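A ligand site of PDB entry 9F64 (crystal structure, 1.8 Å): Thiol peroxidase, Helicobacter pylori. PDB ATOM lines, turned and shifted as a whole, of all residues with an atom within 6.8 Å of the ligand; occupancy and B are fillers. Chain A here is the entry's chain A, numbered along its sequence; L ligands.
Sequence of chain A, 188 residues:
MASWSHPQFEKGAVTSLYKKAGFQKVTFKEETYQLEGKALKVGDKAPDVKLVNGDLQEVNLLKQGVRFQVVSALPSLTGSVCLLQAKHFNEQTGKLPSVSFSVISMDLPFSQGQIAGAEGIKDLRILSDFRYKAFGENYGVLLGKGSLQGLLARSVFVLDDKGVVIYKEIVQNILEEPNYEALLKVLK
The side-chain hydroxyl of Ser 72 sits at hydrogen-bond distance from the guanidinium group of Arg 154 (2.7 Å).
OE1 of Glu 177 lies within salt-bridge range of NH2 of Arg 154, 2.8 Å away.
The backbone carbonyl oxygen of Ala 73 is in hydrogen-bond range of the guanidinium group of Arg 154, at 3.0 Å.
The backbone carbonyl oxygen (O) of Cys 82 lies within hydrogen-bond range of a nitrogen (N3) of the ligand (3.1 Å).
The side-chain sulfur of Cys 82 is bonded to a carbon (C5) of the ligand (1.8 Å).
An oxygen (O1) of the ligand sits at hydrogen-bond distance from the side-chain amide oxygen (OE1) of Gln 85, at 2.6 Å.
A nitrogen (N2) of the ligand lies within hydrogen-bond range of the guanidinium group of Arg 154, 2.7 Å away.
N2 of the ligand is in hydrogen-bond range of OG of Ser 72, at 2.8 Å.
CA of Ala 86 touches N3 of the ligand, 3.5 Å away.
Phe 89 touches the ligand (CG to C2, 3.5 Å).
Phe 101 touches the ligand.
Tyr 180 touches the ligand.
Leu 183 touches the ligand.
Along chain A the residues within 4 Å of the ligand span positions 72 to 183.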
ATOM      1  N   VAL A  70      -3.448  11.393  30.688  1.00  0.00           N
ATOM      2  CA  VAL A  70      -3.589  10.259  29.730  1.00  0.00           C
ATOM      3  C   VAL A  70      -3.157   8.980  30.450  1.00  0.00           C
ATOM      4  O   VAL A  70      -2.023   8.972  30.993  1.00  0.00           O
ATOM      5  CB  VAL A  70      -2.772  10.484  28.449  1.00  0.00           C
ATOM      6  CG1 VAL A  70      -2.935   9.330  27.476  1.00  0.00           C
ATOM      7  CG2 VAL A  70      -3.151  11.796  27.769  1.00  0.00           C
ATOM      8  N   SER A  72      -2.932   4.979  29.517  1.00  0.00           N
ATOM      9  CA  SER A  72      -2.949   3.931  28.460  1.00  0.00           C
ATOM     10  C   SER A  72      -2.640   2.593  29.112  1.00  0.00           C
ATOM     11  O   SER A  72      -1.596   2.516  29.800  1.00  0.00           O
ATOM     12  CB  SER A  72      -1.942   4.238  27.398  1.00  0.00           C
ATOM     13  OG  SER A  72      -1.999   3.257  26.370  1.00  0.00           O
ATOM     14  N   ALA A  73      -3.511   1.594  28.919  1.00  0.00           N
ATOM     15  CA  ALA A  73      -3.354   0.226  29.474  1.00  0.00           C
ATOM     16  C   ALA A  73      -3.185  -0.768  28.322  1.00  0.00           C
ATOM     17  O   ALA A  73      -3.898  -0.623  27.270  1.00  0.00           O
ATOM     18  CB  ALA A  73      -4.510  -0.121  30.375  1.00  0.00           C
ATOM     19  N   LEU A  74      -2.241  -1.704  28.516  1.00  0.00           N
ATOM     20  CA  LEU A  74      -1.784  -2.711  27.521  1.00  0.00           C
ATOM     21  C   LEU A  74      -1.881  -4.090  28.178  1.00  0.00           C
ATOM     22  O   LEU A  74      -1.636  -4.220  29.376  1.00  0.00           O
ATOM     23  CB  LEU A  74      -0.325  -2.440  27.167  1.00  0.00           C
ATOM     24  CG  LEU A  74       0.031  -1.017  26.758  1.00  0.00           C
ATOM     25  CD1 LEU A  74       1.474  -0.695  27.100  1.00  0.00           C
ATOM     26  CD2 LEU A  74      -0.222  -0.817  25.277  1.00  0.00           C
ATOM     27  N   VAL A  81       3.156  -1.766  20.301  1.00  0.00           N
ATOM     28  CA  VAL A  81       3.208  -0.549  19.441  1.00  0.00           C
ATOM     29  C   VAL A  81       3.328   0.688  20.348  1.00  0.00           C
ATOM     30  O   VAL A  81       4.118   1.580  20.017  1.00  0.00           O
ATOM     31  CB  VAL A  81       1.962  -0.450  18.542  1.00  0.00           C
ATOM     32  CG1 VAL A  81       1.934   0.849  17.761  1.00  0.00           C
ATOM     33  CG2 VAL A  81       1.869  -1.642  17.597  1.00  0.00           C
ATOM     34  N   CYS A  82       2.619   0.684  21.476  1.00  0.00           N
ATOM     35  CA  CYS A  82       2.606   1.819  22.405  1.00  0.00           C
ATOM     36  C   CYS A  82       4.020   2.106  22.926  1.00  0.00           C
ATOM     37  O   CYS A  82       4.416   3.262  23.034  1.00  0.00           O
ATOM     38  CB  CYS A  82       1.786   1.481  23.641  1.00  0.00           C
ATOM     39  SG  CYS A  82       1.889   2.833  24.857  1.00  0.00           S
ATOM     40  N   LEU A  83       4.763   1.039  23.229  1.00  0.00           N
ATOM     41  CA  LEU A  83       6.146   1.169  23.755  1.00  0.00           C
ATOM     42  C   LEU A  83       7.027   1.874  22.710  1.00  0.00           C
ATOM     43  O   LEU A  83       7.816   2.741  23.107  1.00  0.00           O
ATOM     44  CB  LEU A  83       6.663  -0.248  24.022  1.00  0.00           C
ATOM     45  CG  LEU A  83       8.177  -0.416  23.939  1.00  0.00           C
ATOM     46  CD1 LEU A  83       8.836   0.112  25.202  1.00  0.00           C
ATOM     47  CD2 LEU A  83       8.552  -1.879  23.716  1.00  0.00           C
ATOM     48  N   LEU A  84       6.860   1.518  21.433  1.00  0.00           N
ATOM     49  CA  LEU A  84       7.663   2.116  20.331  1.00  0.00           C
ATOM     50  C   LEU A  84       7.422   3.622  20.216  1.00  0.00           C
ATOM     51  O   LEU A  84       8.403   4.364  20.036  1.00  0.00           O
ATOM     52  CB  LEU A  84       7.303   1.399  19.023  1.00  0.00           C
ATOM     53  CG  LEU A  84       8.055   0.107  18.741  1.00  0.00           C
ATOM     54  CD1 LEU A  84       8.169  -0.742  20.001  1.00  0.00           C
ATOM     55  CD2 LEU A  84       7.383  -0.685  17.641  1.00  0.00           C
ATOM     56  N   GLN A  85       6.162   4.053  20.334  1.00  0.00           N
ATOM     57  CA  GLN A  85       5.792   5.490  20.173  1.00  0.00           C
ATOM     58  C   GLN A  85       5.716   6.196  21.535  1.00  0.00           C
ATOM     59  O   GLN A  85       5.327   7.380  21.550  1.00  0.00           O
ATOM     60  CB  GLN A  85       4.427   5.586  19.495  1.00  0.00           C
ATOM     61  CG  GLN A  85       4.305   4.740  18.242  1.00  0.00           C
ATOM     62  CD  GLN A  85       2.887   4.687  17.738  1.00  0.00           C
ATOM     63  OE1 GLN A  85       1.952   5.085  18.423  1.00  0.00           O
ATOM     64  NE2 GLN A  85       2.721   4.194  16.526  1.00  0.00           N
ATOM     65  N   ALA A  86       6.075   5.502  22.619  1.00  0.00           N
ATOM     66  CA  ALA A  86       5.957   6.059  23.992  1.00  0.00           C
ATOM     67  C   ALA A  86       6.930   7.227  24.187  1.00  0.00           C
ATOM     68  O   ALA A  86       6.500   8.242  24.768  1.00  0.00           O
ATOM     69  CB  ALA A  86       6.203   4.980  25.008  1.00  0.00           C
ATOM     70  N   LYS A  87       8.184   7.082  23.742  1.00  0.00           N
ATOM     71  CA  LYS A  87       9.240   8.122  23.899  1.00  0.00           C
ATOM     72  C   LYS A  87       8.762   9.414  23.221  1.00  0.00           C
ATOM     73  O   LYS A  87       8.844  10.462  23.878  1.00  0.00           O
ATOM     74  CB  LYS A  87      10.594   7.597  23.395  1.00  0.00           C
ATOM     75  CG  LYS A  87      11.638   8.653  23.059  1.00  0.00           C
ATOM     76  CD  LYS A  87      11.524   9.204  21.653  1.00  0.00           C
ATOM     77  CE  LYS A  87      12.837   9.694  21.088  1.00  0.00           C
ATOM     78  NZ  LYS A  87      12.649  10.410  19.804  1.00  0.00           N
ATOM     79  N   PHE A  89       5.555  10.401  22.146  1.00  0.00           N
ATOM     80  CA  PHE A  89       4.270  10.910  22.683  1.00  0.00           C
ATOM     81  C   PHE A  89       4.514  11.578  24.045  1.00  0.00           C
ATOM     82  O   PHE A  89       3.892  12.620  24.301  1.00  0.00           O
ATOM     83  CB  PHE A  89       3.235   9.790  22.790  1.00  0.00           C
ATOM     84  CG  PHE A  89       1.864  10.256  23.212  1.00  0.00           C
ATOM     85  CD1 PHE A  89       1.005  10.865  22.311  1.00  0.00           C
ATOM     86  CD2 PHE A  89       1.441  10.117  24.532  1.00  0.00           C
ATOM     87  CE1 PHE A  89      -0.249  11.300  22.710  1.00  0.00           C
ATOM     88  CE2 PHE A  89       0.182  10.548  24.924  1.00  0.00           C
ATOM     89  CZ  PHE A  89      -0.654  11.155  24.020  1.00  0.00           C
ATOM     90  N   ASN A  90       5.385  10.981  24.867  1.00  0.00           N
ATOM     91  CA  ASN A  90       5.788  11.484  26.212  1.00  0.00           C
ATOM     92  C   ASN A  90       6.440  12.872  26.079  1.00  0.00           C
ATOM     93  O   ASN A  90       6.164  13.735  26.943  1.00  0.00           O
ATOM     94  CB  ASN A  90       6.720  10.508  26.927  1.00  0.00           C
ATOM     95  CG  ASN A  90       6.912  10.816  28.400  1.00  0.00           C
ATOM     96  OD1 ASN A  90       5.975  11.194  29.094  1.00  0.00           O
ATOM     97  ND2 ASN A  90       8.130  10.636  28.894  1.00  0.00           N
ATOM     98  N   PHE A 101       1.300  11.578  31.104  1.00  0.00           N
ATOM     99  CA  PHE A 101       1.175  10.345  30.303  1.00  0.00           C
ATOM    100  C   PHE A 101       1.646   9.175  31.161  1.00  0.00           C
ATOM    101  O   PHE A 101       2.817   9.196  31.547  1.00  0.00           O
ATOM    102  CB  PHE A 101       1.988  10.450  29.006  1.00  0.00           C
ATOM    103  CG  PHE A 101       1.966   9.219  28.141  1.00  0.00           C
ATOM    104  CD1 PHE A 101       0.785   8.548  27.882  1.00  0.00           C
ATOM    105  CD2 PHE A 101       3.132   8.748  27.546  1.00  0.00           C
ATOM    106  CE1 PHE A 101       0.773   7.403  27.080  1.00  0.00           C
ATOM    107  CE2 PHE A 101       3.123   7.617  26.751  1.00  0.00           C
ATOM    108  CZ  PHE A 101       1.945   6.950  26.514  1.00  0.00           C
ATOM    109  N   VAL A 103       1.581   4.782  31.430  1.00  0.00           N
ATOM    110  CA  VAL A 103       1.375   3.495  30.710  1.00  0.00           C
ATOM    111  C   VAL A 103       1.249   2.415  31.781  1.00  0.00           C
ATOM    112  O   VAL A 103       2.150   2.345  32.664  1.00  0.00           O
ATOM    113  CB  VAL A 103       2.511   3.227  29.708  1.00  0.00           C
ATOM    114  CG1 VAL A 103       2.342   1.883  29.021  1.00  0.00           C
ATOM    115  CG2 VAL A 103       2.560   4.351  28.663  1.00  0.00           C
ATOM    116  N   LEU A 124       9.690   7.730  31.607  1.00  0.00           N
ATOM    117  CA  LEU A 124       8.294   7.496  31.184  1.00  0.00           C
ATOM    118  C   LEU A 124       7.590   6.903  32.392  1.00  0.00           C
ATOM    119  O   LEU A 124       8.212   6.103  33.086  1.00  0.00           O
ATOM    120  CB  LEU A 124       8.291   6.545  29.974  1.00  0.00           C
ATOM    121  CG  LEU A 124       6.912   6.081  29.535  1.00  0.00           C
ATOM    122  CD1 LEU A 124       6.024   7.257  29.207  1.00  0.00           C
ATOM    123  CD2 LEU A 124       7.012   5.155  28.344  1.00  0.00           C
ATOM    124  N   ARG A 154      -6.551  -3.522  25.965  1.00  0.00           N
ATOM    125  CA  ARG A 154      -5.971  -2.320  25.318  1.00  0.00           C
ATOM    126  C   ARG A 154      -6.997  -1.190  25.449  1.00  0.00           C
ATOM    127  O   ARG A 154      -8.121  -1.377  24.987  1.00  0.00           O
ATOM    128  CB  ARG A 154      -5.651  -2.546  23.836  1.00  0.00           C
ATOM    129  CG  ARG A 154      -4.865  -1.405  23.204  1.00  0.00           C
ATOM    130  CD  ARG A 154      -3.453  -1.341  23.720  1.00  0.00           C
ATOM    131  NE  ARG A 154      -2.712  -0.195  23.210  1.00  0.00           N
ATOM    132  CZ  ARG A 154      -2.576   0.971  23.833  1.00  0.00           C
ATOM    133  NH1 ARG A 154      -3.127   1.174  25.025  1.00  0.00           N
ATOM    134  NH2 ARG A 154      -1.869   1.940  23.273  1.00  0.00           N
ATOM    135  N   SER A 155      -6.613  -0.110  26.117  1.00  0.00           N
ATOM    136  CA  SER A 155      -7.549   0.981  26.496  1.00  0.00           C
ATOM    137  C   SER A 155      -6.771   2.276  26.736  1.00  0.00           C
ATOM    138  O   SER A 155      -5.554   2.241  27.006  1.00  0.00           O
ATOM    139  CB  SER A 155      -8.372   0.595  27.701  1.00  0.00           C
ATOM    140  OG  SER A 155      -7.544   0.139  28.774  1.00  0.00           O
ATOM    141  N   VAL A 156      -7.454   3.406  26.586  1.00  0.00           N
ATOM    142  CA  VAL A 156      -6.877   4.730  26.937  1.00  0.00           C
ATOM    143  C   VAL A 156      -7.998   5.543  27.601  1.00  0.00           C
ATOM    144  O   VAL A 156      -9.178   5.399  27.191  1.00  0.00           O
ATOM    145  CB  VAL A 156      -6.275   5.436  25.709  1.00  0.00           C
ATOM    146  CG1 VAL A 156      -7.319   5.765  24.662  1.00  0.00           C
ATOM    147  CG2 VAL A 156      -5.482   6.677  26.115  1.00  0.00           C
ATOM    148  N   GLU A 177      -4.402  -0.572  18.011  1.00  0.00           N
ATOM    149  CA  GLU A 177      -4.065   0.638  18.794  1.00  0.00           C
ATOM    150  C   GLU A 177      -5.315   1.503  18.959  1.00  0.00           C
ATOM    151  O   GLU A 177      -6.222   1.411  18.130  1.00  0.00           O
ATOM    152  CB  GLU A 177      -2.941   1.422  18.113  1.00  0.00           C
ATOM    153  CG  GLU A 177      -1.561   0.857  18.400  1.00  0.00           C
ATOM    154  CD  GLU A 177      -1.312   0.624  19.883  1.00  0.00           C
ATOM    155  OE1 GLU A 177      -1.013   1.609  20.586  1.00  0.00           O
ATOM    156  OE2 GLU A 177      -1.459  -0.537  20.336  1.00  0.00           O
ATOM    157  N   PRO A 178      -5.408   2.308  20.036  1.00  0.00           N
ATOM    158  CA  PRO A 178      -6.502   3.273  20.190  1.00  0.00           C
ATOM    159  C   PRO A 178      -6.493   4.318  19.063  1.00  0.00           C
ATOM    160  O   PRO A 178      -5.457   4.510  18.427  1.00  0.00           O
ATOM    161  CB  PRO A 178      -6.232   3.927  21.550  1.00  0.00           C
ATOM    162  CG  PRO A 178      -5.334   2.933  22.283  1.00  0.00           C
ATOM    163  CD  PRO A 178      -4.496   2.304  21.186  1.00  0.00           C
ATOM    164  N   ASN A 179      -7.636   4.956  18.844  1.00  0.00           N
ATOM    165  CA  ASN A 179      -7.846   6.038  17.840  1.00  0.00           C
ATOM    166  C   ASN A 179      -6.906   7.196  18.168  1.00  0.00           C
ATOM    167  O   ASN A 179      -7.117   7.844  19.223  1.00  0.00           O
ATOM    168  CB  ASN A 179      -9.294   6.502  17.798  1.00  0.00           C
ATOM    169  CG  ASN A 179      -9.573   7.360  16.579  1.00  0.00           C
ATOM    170  OD1 ASN A 179      -8.949   8.415  16.400  1.00  0.00           O
ATOM    171  ND2 ASN A 179     -10.481   6.914  15.730  1.00  0.00           N
ATOM    172  N   TYR A 180      -5.914   7.456  17.317  1.00  0.00           N
ATOM    173  CA  TYR A 180      -4.846   8.452  17.574  1.00  0.00           C
ATOM    174  C   TYR A 180      -5.424   9.858  17.422  1.00  0.00           C
ATOM    175  O   TYR A 180      -5.224  10.723  18.296  1.00  0.00           O
ATOM    176  CB  TYR A 180      -3.678   8.254  16.612  1.00  0.00           C
ATOM    177  CG  TYR A 180      -2.443   9.037  17.010  1.00  0.00           C
ATOM    178  CD1 TYR A 180      -1.816   9.899  16.119  1.00  0.00           C
ATOM    179  CD2 TYR A 180      -1.933   8.938  18.286  1.00  0.00           C
ATOM    180  CE1 TYR A 180      -0.699  10.620  16.485  1.00  0.00           C
ATOM    181  CE2 TYR A 180      -0.810   9.654  18.675  1.00  0.00           C
ATOM    182  CZ  TYR A 180      -0.191  10.500  17.771  1.00  0.00           C
ATOM    183  OH  TYR A 180       0.914  11.201  18.166  1.00  0.00           O
ATOM    184  N   LEU A 183      -7.689  10.935  20.308  1.00  0.00           N
ATOM    185  CA  LEU A 183      -6.924  11.165  21.555  1.00  0.00           C
ATOM    186  C   LEU A 183      -6.260  12.537  21.498  1.00  0.00           C
ATOM    187  O   LEU A 183      -6.365  13.286  22.513  1.00  0.00           O
ATOM    188  CB  LEU A 183      -5.866  10.070  21.726  1.00  0.00           C
ATOM    189  CG  LEU A 183      -4.944  10.318  22.914  1.00  0.00           C
ATOM    190  CD1 LEU A 183      -5.755  10.465  24.191  1.00  0.00           C
ATOM    191  CD2 LEU A 183      -3.916   9.216  23.032  1.00  0.00           C
HETATM  192  O1  LIG L   1       1.382   6.457  20.561  1.00  0.00           O
HETATM  193  C1  LIG L   1       0.172   7.090  20.995  1.00  0.00           C
HETATM  194  C2  LIG L   1       0.158   7.236  22.514  1.00  0.00           C
HETATM  195  N1  LIG L   1       0.217   5.921  23.200  1.00  0.00           N
HETATM  196  C3  LIG L   1      -0.843   5.203  23.560  1.00  0.00           C
HETATM  197  C4  LIG L   1      -2.294   5.597  23.339  1.00  0.00           C
HETATM  198  N2  LIG L   1      -0.453   4.071  24.150  1.00  0.00           N
HETATM  199  C5  LIG L   1       0.859   4.122  24.173  1.00  0.00           C
HETATM  200  C6  LIG L   1       1.284   5.232  23.585  1.00  0.00           C
HETATM  201  N3  LIG L   1       2.511   5.664  23.367  1.00  0.00           N
